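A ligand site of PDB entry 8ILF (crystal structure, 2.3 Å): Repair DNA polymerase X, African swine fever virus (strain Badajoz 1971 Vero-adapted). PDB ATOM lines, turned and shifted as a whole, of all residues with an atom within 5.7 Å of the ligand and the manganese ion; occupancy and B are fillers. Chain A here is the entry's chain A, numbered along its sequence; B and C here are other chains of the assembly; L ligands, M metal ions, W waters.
The backbone NH of Ser 43 lies close to an oxygen (O6) of the ligand.
OG of Ser 43 sits at hydrogen-bond distance from O2 of the ligand, 2.6 Å away.
N1 of DA 9 of chain B sits close to a nitrogen (N4) of the ligand, at 3.5 Å.
N3 of DC 1 of chain C lies within hydrogen-bond range of N4 of the ligand (2.9 Å).
NH1 of Arg 46 lies within salt-bridge range of O5 of the ligand, at 3.0 Å.
The backbone NH (N) of Asn 52 lies within hydrogen-bond range of an oxygen (O2) of the ligand, at 3.1 Å.
The side-chain amide oxygen of Asn 52 sits close to an oxygen (O3) of the ligand.
An oxygen (O11) of the ligand is in hydrogen-bond range of the backbone carbonyl oxygen of Phe 120 (3.1 Å).
O11 of the ligand sits at hydrogen-bond distance from O of Thr 121.
The backbone carbonyl oxygen (O) of Asp 55 lies within hydrogen-bond range of the backbone NH (N) of Val 41 (3.0 Å).
O2 of DC 1 of chain C lies within hydrogen-bond range of the guanidinium group of Arg 131 (3.2 Å).
The guanidinium group (NH1) of Arg 46 lies within hydrogen-bond range of the backbone carbonyl oxygen (O) of Thr 121 (2.8 Å).
The backbone carbonyl oxygen of Phe 120 is in hydrogen-bond range of the backbone NH of Gly 42.
A ring nitrogen (ND1) of His 119 sits at hydrogen-bond distance from the guanidinium group of Arg 131, 3.2 Å away.
The guanidinium group (NH1) of Arg 131 sits at hydrogen-bond distance from O4' of DT 2 of chain C (3.4 Å).
NH1 of Arg 131 sits close to N3 of the ligand, at 3.2 Å.
Gly 42 touches the ligand (CA to O6, 3.4 Å).
Leu 51 touches the ligand (CA to O2, 3.8 Å).
His 119 touches the ligand (O to C4, 3.2 Å).
Gly 122 touches the ligand.
CG2 of Val 124 touches C9 of the ligand, 3.2 Å away.
CD1 of Leu 127 touches N2 of the ligand (3.5 Å).
DT 2 of chain C touches the ligand (O2 to N3, 3.7 Å).
Within 4 Å of the ligand: Gly 42, Ser 43, Arg 46, Leu 51, Asn 52, Asp 53, Asp 55, His 119, Phe 120, Thr 121, Gly 122, Val 124, Leu 127, Arg 131, DA 9 of chain B, DC 1 of chain C and DT 2 of chain C.
The nearest printed residue that does not touch the ligand is Met 50 (4.2 Å).
Residues that only touch the manganese ion: Ser 43 (3.97 Å).
Of the 24 residues printed, 3 come within 4 Å of the manganese ion.
Along chain A the residues within 4 Å of the manganese ion span positions 43 to 55.
The manganese ion is bound by an oxygen (O1) of the ligand (2.0 Å), the side-chain carboxylate of Asp 53 (2.1 Å), an oxygen (O8) of the ligand (2.1 Å), the side-chain carboxylate of Asp 55 (2.1 Å), an oxygen (O6) of the ligand (2.2 Å) and water W2 (2.2 Å).
Water W2 lies within hydrogen-bond range of OG of Ser 43 (2.6 Å) and O of Asp 53 (2.7 Å).
Water W1 lies within hydrogen-bond range of the backbone NH (N) of Val 124 (3.1 Å) and an oxygen (O5) of the ligand (3.2 Å).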
ATOM      1  N   VAL A  41      30.277   9.667   0.292  1.00  0.00           N
ATOM      2  CA  VAL A  41      28.979  10.315   0.095  1.00  0.00           C
ATOM      3  C   VAL A  41      28.023   9.741   1.148  1.00  0.00           C
ATOM      4  O   VAL A  41      28.483   9.138   2.109  1.00  0.00           O
ATOM      5  CB  VAL A  41      28.482  10.183  -1.370  1.00  0.00           C
ATOM      6  CG1 VAL A  41      29.354  11.022  -2.301  1.00  0.00           C
ATOM      7  CG2 VAL A  41      28.455   8.733  -1.843  1.00  0.00           C
ATOM      8  N   GLY A  42      26.721   9.957   1.004  1.00  0.00           N
ATOM      9  CA  GLY A  42      25.735   9.387   1.896  1.00  0.00           C
ATOM     10  C   GLY A  42      25.820   9.995   3.284  1.00  0.00           C
ATOM     11  O   GLY A  42      26.286  11.117   3.440  1.00  0.00           O
ATOM     12  N   SER A  43      25.379   9.252   4.287  1.00  0.00           N
ATOM     13  CA  SER A  43      25.284   9.792   5.641  1.00  0.00           C
ATOM     14  C   SER A  43      26.675  10.081   6.247  1.00  0.00           C
ATOM     15  O   SER A  43      26.782  10.927   7.100  1.00  0.00           O
ATOM     16  CB  SER A  43      24.406   8.912   6.542  1.00  0.00           C
ATOM     17  OG  SER A  43      24.748   7.537   6.476  1.00  0.00           O
ATOM     18  N   LEU A  44      27.725   9.415   5.765  1.00  0.00           N
ATOM     19  CA  LEU A  44      29.084   9.704   6.219  1.00  0.00           C
ATOM     20  C   LEU A  44      29.565  11.095   5.826  1.00  0.00           C
ATOM     21  O   LEU A  44      30.143  11.799   6.667  1.00  0.00           O
ATOM     22  CB  LEU A  44      30.065   8.649   5.686  1.00  0.00           C
ATOM     23  CG  LEU A  44      31.565   8.837   5.908  1.00  0.00           C
ATOM     24  CD1 LEU A  44      31.924   9.114   7.346  1.00  0.00           C
ATOM     25  CD2 LEU A  44      32.276   7.581   5.447  1.00  0.00           C
ATOM     26  N   ARG A  46      27.712  13.609   5.259  1.00  0.00           N
ATOM     27  CA  ARG A  46      26.862  14.458   6.070  1.00  0.00           C
ATOM     28  C   ARG A  46      27.176  14.433   7.593  1.00  0.00           C
ATOM     29  O   ARG A  46      26.519  15.112   8.365  1.00  0.00           O
ATOM     30  CB  ARG A  46      25.400  14.089   5.830  1.00  0.00           C
ATOM     31  CG  ARG A  46      24.897  14.312   4.406  1.00  0.00           C
ATOM     32  CD  ARG A  46      23.386  14.492   4.365  1.00  0.00           C
ATOM     33  NE  ARG A  46      22.716  13.459   5.159  1.00  0.00           N
ATOM     34  CZ  ARG A  46      22.399  12.223   4.770  1.00  0.00           C
ATOM     35  NH1 ARG A  46      22.652  11.780   3.522  1.00  0.00           N
ATOM     36  NH2 ARG A  46      21.788  11.408   5.626  1.00  0.00           N
ATOM     37  N   MET A  50      25.160   8.157  13.502  1.00  0.00           N
ATOM     38  CA  MET A  50      24.764   6.770  13.160  1.00  0.00           C
ATOM     39  C   MET A  50      24.742   6.570  11.644  1.00  0.00           C
ATOM     40  O   MET A  50      24.147   7.367  10.929  1.00  0.00           O
ATOM     41  CB  MET A  50      23.361   6.479  13.679  1.00  0.00           C
ATOM     42  CG  MET A  50      23.154   6.832  15.144  1.00  0.00           C
ATOM     43  SD  MET A  50      21.592   6.172  15.753  1.00  0.00           S
ATOM     44  CE  MET A  50      20.435   7.265  14.909  1.00  0.00           C
ATOM     45  N   LEU A  51      25.348   5.475  11.176  1.00  0.00           N
ATOM     46  CA  LEU A  51      25.395   5.114   9.754  1.00  0.00           C
ATOM     47  C   LEU A  51      24.850   3.692   9.577  1.00  0.00           C
ATOM     48  O   LEU A  51      25.277   2.771  10.298  1.00  0.00           O
ATOM     49  CB  LEU A  51      26.829   5.151   9.233  1.00  0.00           C
ATOM     50  CG  LEU A  51      27.676   6.380   9.536  1.00  0.00           C
ATOM     51  CD1 LEU A  51      29.115   6.135   9.106  1.00  0.00           C
ATOM     52  CD2 LEU A  51      27.096   7.633   8.876  1.00  0.00           C
ATOM     53  N   ASN A  52      23.939   3.507   8.628  1.00  0.00           N
ATOM     54  CA  ASN A  52      23.508   2.146   8.246  1.00  0.00           C
ATOM     55  C   ASN A  52      24.473   1.444   7.263  1.00  0.00           C
ATOM     56  O   ASN A  52      24.383   0.228   7.061  1.00  0.00           O
ATOM     57  CB  ASN A  52      22.078   2.157   7.691  1.00  0.00           C
ATOM     58  CG  ASN A  52      21.054   2.549   8.761  1.00  0.00           C
ATOM     59  OD1 ASN A  52      20.369   3.556   8.642  1.00  0.00           O
ATOM     60  ND2 ASN A  52      20.967   1.760   9.819  1.00  0.00           N
ATOM     61  N   ASP A  53      25.393   2.203   6.669  1.00  0.00           N
ATOM     62  CA  ASP A  53      26.309   1.675   5.651  1.00  0.00           C
ATOM     63  C   ASP A  53      27.328   2.743   5.287  1.00  0.00           C
ATOM     64  O   ASP A  53      27.202   3.892   5.728  1.00  0.00           O
ATOM     65  CB  ASP A  53      25.540   1.240   4.403  1.00  0.00           C
ATOM     66  CG  ASP A  53      24.510   2.263   3.980  1.00  0.00           C
ATOM     67  OD1 ASP A  53      24.911   3.350   3.529  1.00  0.00           O
ATOM     68  OD2 ASP A  53      23.293   1.973   4.129  1.00  0.00           O
ATOM     69  N   VAL A  54      28.316   2.353   4.491  1.00  0.00           N
ATOM     70  CA  VAL A  54      29.292   3.293   3.966  1.00  0.00           C
ATOM     71  C   VAL A  54      29.110   3.394   2.461  1.00  0.00           C
ATOM     72  O   VAL A  54      29.227   2.378   1.766  1.00  0.00           O
ATOM     73  CB  VAL A  54      30.725   2.835   4.271  1.00  0.00           C
ATOM     74  CG1 VAL A  54      31.754   3.793   3.661  1.00  0.00           C
ATOM     75  CG2 VAL A  54      30.912   2.713   5.771  1.00  0.00           C
ATOM     76  N   ASP A  55      28.850   4.600   1.967  1.00  0.00           N
ATOM     77  CA  ASP A  55      28.643   4.882   0.543  1.00  0.00           C
ATOM     78  C   ASP A  55      29.863   5.600  -0.031  1.00  0.00           C
ATOM     79  O   ASP A  55      30.254   6.663   0.497  1.00  0.00           O
ATOM     80  CB  ASP A  55      27.415   5.766   0.362  1.00  0.00           C
ATOM     81  CG  ASP A  55      26.166   5.193   1.024  1.00  0.00           C
ATOM     82  OD1 ASP A  55      25.698   4.125   0.565  1.00  0.00           O
ATOM     83  OD2 ASP A  55      25.641   5.803   1.976  1.00  0.00           O
ATOM     84  N   ASP A 104      28.529   0.366   0.005  1.00  0.00           N
ATOM     85  CA  ASP A 104      27.898   0.675  -1.257  1.00  0.00           C
ATOM     86  C   ASP A 104      28.872   1.450  -2.122  1.00  0.00           C
ATOM     87  O   ASP A 104      29.446   2.441  -1.670  1.00  0.00           O
ATOM     88  CB  ASP A 104      26.629   1.493  -1.042  1.00  0.00           C
ATOM     89  CG  ASP A 104      25.578   0.755  -0.243  1.00  0.00           C
ATOM     90  OD1 ASP A 104      25.618  -0.496  -0.218  1.00  0.00           O
ATOM     91  OD2 ASP A 104      24.711   1.403   0.381  1.00  0.00           O
ATOM     92  N   PHE A 106      29.350   3.293  -5.956  1.00  0.00           N
ATOM     93  CA  PHE A 106      28.594   3.872  -7.065  1.00  0.00           C
ATOM     94  C   PHE A 106      29.609   4.422  -8.044  1.00  0.00           C
ATOM     95  O   PHE A 106      30.733   4.752  -7.641  1.00  0.00           O
ATOM     96  CB  PHE A 106      27.684   4.991  -6.580  1.00  0.00           C
ATOM     97  CG  PHE A 106      26.742   4.593  -5.477  1.00  0.00           C
ATOM     98  CD1 PHE A 106      25.520   3.985  -5.774  1.00  0.00           C
ATOM     99  CD2 PHE A 106      27.071   4.817  -4.153  1.00  0.00           C
ATOM    100  CE1 PHE A 106      24.638   3.616  -4.761  1.00  0.00           C
ATOM    101  CE2 PHE A 106      26.207   4.442  -3.134  1.00  0.00           C
ATOM    102  CZ  PHE A 106      24.987   3.843  -3.427  1.00  0.00           C
ATOM    103  N   HIS A 119      23.599  14.219  -5.744  1.00  0.00           N
ATOM    104  CA  HIS A 119      22.586  13.199  -5.601  1.00  0.00           C
ATOM    105  C   HIS A 119      22.923  12.282  -4.421  1.00  0.00           C
ATOM    106  O   HIS A 119      22.100  12.085  -3.512  1.00  0.00           O
ATOM    107  CB  HIS A 119      22.444  12.417  -6.930  1.00  0.00           C
ATOM    108  CG  HIS A 119      21.769  11.088  -6.817  1.00  0.00           C
ATOM    109  ND1 HIS A 119      20.412  10.921  -6.981  1.00  0.00           N
ATOM    110  CD2 HIS A 119      22.273   9.853  -6.586  1.00  0.00           C
ATOM    111  CE1 HIS A 119      20.113   9.637  -6.850  1.00  0.00           C
ATOM    112  NE2 HIS A 119      21.225   8.981  -6.597  1.00  0.00           N
ATOM    113  N   PHE A 120      24.147  11.759  -4.381  1.00  0.00           N
ATOM    114  CA  PHE A 120      24.486  10.744  -3.399  1.00  0.00           C
ATOM    115  C   PHE A 120      24.757  11.289  -2.012  1.00  0.00           C
ATOM    116  O   PHE A 120      24.801  10.533  -1.059  1.00  0.00           O
ATOM    117  CB  PHE A 120      25.642   9.859  -3.872  1.00  0.00           C
ATOM    118  CG  PHE A 120      25.248   8.877  -4.925  1.00  0.00           C
ATOM    119  CD1 PHE A 120      24.354   7.858  -4.626  1.00  0.00           C
ATOM    120  CD2 PHE A 120      25.753   8.970  -6.229  1.00  0.00           C
ATOM    121  CE1 PHE A 120      23.978   6.941  -5.588  1.00  0.00           C
ATOM    122  CE2 PHE A 120      25.382   8.057  -7.200  1.00  0.00           C
ATOM    123  CZ  PHE A 120      24.495   7.040  -6.886  1.00  0.00           C
ATOM    124  N   THR A 121      24.940  12.604  -1.894  1.00  0.00           N
ATOM    125  CA  THR A 121      25.094  13.248  -0.589  1.00  0.00           C
ATOM    126  C   THR A 121      23.761  13.315   0.166  1.00  0.00           C
ATOM    127  O   THR A 121      23.747  13.143   1.387  1.00  0.00           O
ATOM    128  CB  THR A 121      25.752  14.635  -0.722  1.00  0.00           C
ATOM    129  OG1 THR A 121      27.102  14.427  -1.142  1.00  0.00           O
ATOM    130  CG2 THR A 121      25.740  15.391   0.611  1.00  0.00           C
ATOM    131  N   GLY A 122      22.655  13.521  -0.544  1.00  0.00           N
ATOM    132  CA  GLY A 122      21.338  13.557   0.079  1.00  0.00           C
ATOM    133  C   GLY A 122      21.264  14.699   1.082  1.00  0.00           C
ATOM    134  O   GLY A 122      21.954  15.693   0.882  1.00  0.00           O
ATOM    135  N   PRO A 123      20.450  14.596   2.146  1.00  0.00           N
ATOM    136  CA  PRO A 123      19.492  13.490   2.372  1.00  0.00           C
ATOM    137  C   PRO A 123      18.352  13.515   1.371  1.00  0.00           C
ATOM    138  O   PRO A 123      18.219  14.491   0.613  1.00  0.00           O
ATOM    139  CB  PRO A 123      18.960  13.774   3.774  1.00  0.00           C
ATOM    140  CG  PRO A 123      19.031  15.271   3.892  1.00  0.00           C
ATOM    141  CD  PRO A 123      20.179  15.736   3.030  1.00  0.00           C
ATOM    142  N   VAL A 124      17.548  12.464   1.362  1.00  0.00           N
ATOM    143  CA  VAL A 124      16.490  12.322   0.366  1.00  0.00           C
ATOM    144  C   VAL A 124      15.525  13.499   0.469  1.00  0.00           C
ATOM    145  O   VAL A 124      15.200  14.090  -0.554  1.00  0.00           O
ATOM    146  CB  VAL A 124      15.760  10.961   0.478  1.00  0.00           C
ATOM    147  CG1 VAL A 124      14.522  10.922  -0.416  1.00  0.00           C
ATOM    148  CG2 VAL A 124      16.702   9.831   0.096  1.00  0.00           C
ATOM    149  N   LEU A 127      16.783  16.419  -1.336  1.00  0.00           N
ATOM    150  CA  LEU A 127      16.767  16.205  -2.775  1.00  0.00           C
ATOM    151  C   LEU A 127      15.373  16.369  -3.383  1.00  0.00           C
ATOM    152  O   LEU A 127      15.254  16.884  -4.484  1.00  0.00           O
ATOM    153  CB  LEU A 127      17.322  14.830  -3.153  1.00  0.00           C
ATOM    154  CG  LEU A 127      18.800  14.556  -2.851  1.00  0.00           C
ATOM    155  CD1 LEU A 127      19.140  13.167  -3.338  1.00  0.00           C
ATOM    156  CD2 LEU A 127      19.736  15.590  -3.460  1.00  0.00           C
ATOM    157  N   ARG A 131      14.470  19.102  -6.272  1.00  0.00           N
ATOM    158  CA  ARG A 131      14.035  18.536  -7.541  1.00  0.00           C
ATOM    159  C   ARG A 131      12.639  19.013  -7.950  1.00  0.00           C
ATOM    160  O   ARG A 131      12.418  19.279  -9.121  1.00  0.00           O
ATOM    161  CB  ARG A 131      14.150  17.011  -7.543  1.00  0.00           C
ATOM    162  CG  ARG A 131      15.609  16.573  -7.600  1.00  0.00           C
ATOM    163  CD  ARG A 131      15.839  15.095  -7.373  1.00  0.00           C
ATOM    164  NE  ARG A 131      17.269  14.847  -7.554  1.00  0.00           N
ATOM    165  CZ  ARG A 131      17.837  13.700  -7.920  1.00  0.00           C
ATOM    166  NH1 ARG A 131      17.122  12.596  -8.142  1.00  0.00           N
ATOM    167  NH2 ARG A 131      19.163  13.676  -8.072  1.00  0.00           N
ATOM    168  P    DA B   9      20.503  -1.324  -1.447  1.00  0.00           P
ATOM    169  OP1  DA B   9      21.212  -2.336  -2.278  1.00  0.00           O
ATOM    170  OP2  DA B   9      20.803  -1.192   0.013  1.00  0.00           O
ATOM    171  O5'  DA B   9      20.727   0.100  -2.123  1.00  0.00           O
ATOM    172  C5'  DA B   9      21.034   1.281  -1.355  1.00  0.00           C
ATOM    173  C4'  DA B   9      21.396   2.400  -2.307  1.00  0.00           C
ATOM    174  O4'  DA B   9      20.389   2.491  -3.342  1.00  0.00           O
ATOM    175  C3'  DA B   9      21.469   3.793  -1.686  1.00  0.00           C
ATOM    176  C2'  DA B   9      21.111   4.689  -2.860  1.00  0.00           C
ATOM    177  C1'  DA B   9      20.133   3.845  -3.674  1.00  0.00           C
ATOM    178  N9   DA B   9      18.706   4.092  -3.468  1.00  0.00           N
ATOM    179  C8   DA B   9      17.883   3.520  -2.529  1.00  0.00           C
ATOM    180  N7   DA B   9      16.631   3.891  -2.617  1.00  0.00           N
ATOM    181  C5   DA B   9      16.624   4.761  -3.707  1.00  0.00           C
ATOM    182  C6   DA B   9      15.589   5.485  -4.327  1.00  0.00           C
ATOM    183  N6   DA B   9      14.323   5.462  -3.912  1.00  0.00           N
ATOM    184  N1   DA B   9      15.923   6.261  -5.376  1.00  0.00           N
ATOM    185  C2   DA B   9      17.201   6.298  -5.779  1.00  0.00           C
ATOM    186  N3   DA B   9      18.256   5.651  -5.283  1.00  0.00           N
ATOM    187  C4   DA B   9      17.896   4.885  -4.242  1.00  0.00           C
ATOM    188  O5'  DC C   1       8.863  14.574  -6.403  1.00  0.00           O
ATOM    189  C5'  DC C   1       9.651  15.751  -6.675  1.00  0.00           C
ATOM    190  C4'  DC C   1      10.987  15.352  -7.279  1.00  0.00           C
ATOM    191  O4'  DC C   1      11.729  14.538  -6.334  1.00  0.00           O
ATOM    192  C3'  DC C   1      10.886  14.532  -8.570  1.00  0.00           C
ATOM    193  O3'  DC C   1      11.747  15.060  -9.577  1.00  0.00           O
ATOM    194  C2'  DC C   1      11.299  13.136  -8.151  1.00  0.00           C
ATOM    195  C1'  DC C   1      12.240  13.395  -6.989  1.00  0.00           C
ATOM    196  N1   DC C   1      12.277  12.308  -6.003  1.00  0.00           N
ATOM    197  C2   DC C   1      13.488  11.645  -5.756  1.00  0.00           C
ATOM    198  O2   DC C   1      14.502  12.013  -6.355  1.00  0.00           O
ATOM    199  N3   DC C   1      13.509  10.634  -4.852  1.00  0.00           N
ATOM    200  C4   DC C   1      12.397  10.268  -4.213  1.00  0.00           C
ATOM    201  N4   DC C   1      12.466   9.274  -3.340  1.00  0.00           N
ATOM    202  C5   DC C   1      11.149  10.926  -4.454  1.00  0.00           C
ATOM    203  C6   DC C   1      11.133  11.930  -5.348  1.00  0.00           C
ATOM    204  P    DT C   2      11.565  14.619 -11.105  1.00  0.00           P
ATOM    205  OP1  DT C   2      12.047  15.729 -11.951  1.00  0.00           O
ATOM    206  OP2  DT C   2      10.195  14.090 -11.287  1.00  0.00           O
ATOM    207  O5'  DT C   2      12.551  13.377 -11.246  1.00  0.00           O
ATOM    208  C5'  DT C   2      13.948  13.526 -10.944  1.00  0.00           C
ATOM    209  C4'  DT C   2      14.603  12.163 -10.894  1.00  0.00           C
ATOM    210  O4'  DT C   2      14.248  11.516  -9.655  1.00  0.00           O
ATOM    211  C3'  DT C   2      14.183  11.190 -12.000  1.00  0.00           C
ATOM    212  O3'  DT C   2      15.266  11.054 -12.923  1.00  0.00           O
ATOM    213  C2'  DT C   2      13.808   9.916 -11.263  1.00  0.00           C
ATOM    214  C1'  DT C   2      14.418  10.135  -9.889  1.00  0.00           C
ATOM    215  N1   DT C   2      13.818   9.389  -8.759  1.00  0.00           N
ATOM    216  C2   DT C   2      14.672   8.705  -7.925  1.00  0.00           C
ATOM    217  O2   DT C   2      15.893   8.714  -8.053  1.00  0.00           O
ATOM    218  N3   DT C   2      14.061   8.010  -6.919  1.00  0.00           N
ATOM    219  C4   DT C   2      12.700   7.920  -6.675  1.00  0.00           C
ATOM    220  O4   DT C   2      12.292   7.246  -5.735  1.00  0.00           O
ATOM    221  C5   DT C   2      11.860   8.665  -7.596  1.00  0.00           C
ATOM    222  C7   DT C   2      10.372   8.639  -7.405  1.00  0.00           C
ATOM    223  C6   DT C   2      12.460   9.350  -8.575  1.00  0.00           C
HETATM  224  O1  LIG L   1      22.847   4.925   4.890  1.00  0.00           O
HETATM  225  P1  LIG L   1      22.039   5.727   5.875  1.00  0.00           P
HETATM  226  O2  LIG L   1      22.733   5.976   7.192  1.00  0.00           O
HETATM  227  O3  LIG L   1      20.630   5.163   6.045  1.00  0.00           O
HETATM  228  O4  LIG L   1      21.804   7.203   5.252  1.00  0.00           O
HETATM  229  P2  LIG L   1      22.027   7.623   3.697  1.00  0.00           P
HETATM  230  O5  LIG L   1      21.538   9.045   3.567  1.00  0.00           O
HETATM  231  O6  LIG L   1      23.459   7.306   3.351  1.00  0.00           O
HETATM  232  O7  LIG L   1      20.945   6.679   2.928  1.00  0.00           O
HETATM  233  P3  LIG L   1      21.157   5.548   1.768  1.00  0.00           P
HETATM  234 SE1  LIG L   1      19.457   4.637   1.495  1.00  0.00          SE
HETATM  235  O8  LIG L   1      22.414   4.816   2.112  1.00  0.00           O
HETATM  236  O9  LIG L   1      21.397   6.484   0.521  1.00  0.00           O
HETATM  237  C1  LIG L   1      22.681   6.937   0.117  1.00  0.00           C
HETATM  238  C2  LIG L   1      22.495   8.175  -0.738  1.00  0.00           C
HETATM  239  O10 LIG L   1      21.914   7.776  -1.983  1.00  0.00           O
HETATM  240  C3  LIG L   1      21.573   9.261  -0.179  1.00  0.00           C
HETATM  241  O11 LIG L   1      22.245  10.188   0.650  1.00  0.00           O
HETATM  242  C4  LIG L   1      21.041   9.909  -1.441  1.00  0.00           C
HETATM  243  C5  LIG L   1      20.947   8.748  -2.421  1.00  0.00           C
HETATM  244  N1  LIG L   1      19.554   8.283  -2.299  1.00  0.00           N
HETATM  245  C6  LIG L   1      18.555   8.812  -2.978  1.00  0.00           C
HETATM  246  N2  LIG L   1      18.445   9.745  -3.939  1.00  0.00           N
HETATM  247  C7  LIG L   1      17.235  10.057  -4.469  1.00  0.00           C
HETATM  248  N3  LIG L   1      17.184  11.007  -5.421  1.00  0.00           N
HETATM  249  N4  LIG L   1      16.077   9.463  -4.064  1.00  0.00           N
HETATM  250  C8  LIG L   1      19.072   7.368  -1.437  1.00  0.00           C
HETATM  251  N5  LIG L   1      17.734   7.242  -1.578  1.00  0.00           N
HETATM  252  C9  LIG L   1      17.353   8.111  -2.518  1.00  0.00           C
HETATM  253  C10 LIG L   1      16.074   8.514  -3.112  1.00  0.00           C
HETATM  254  O12 LIG L   1      15.032   7.944  -2.740  1.00  0.00           O
HETATM  255 MN    MN M   1      24.075   5.238   3.312  1.00  0.00          MN
HETATM  256  O   HOH W   1      18.567   9.944   2.848  1.00  0.00           O
HETATM  257  O   HOH W   2      25.677   5.902   4.741  1.00  0.00           O
HETATM  258  O   HOH W   3      16.105   5.889   0.400  1.00  0.00           O
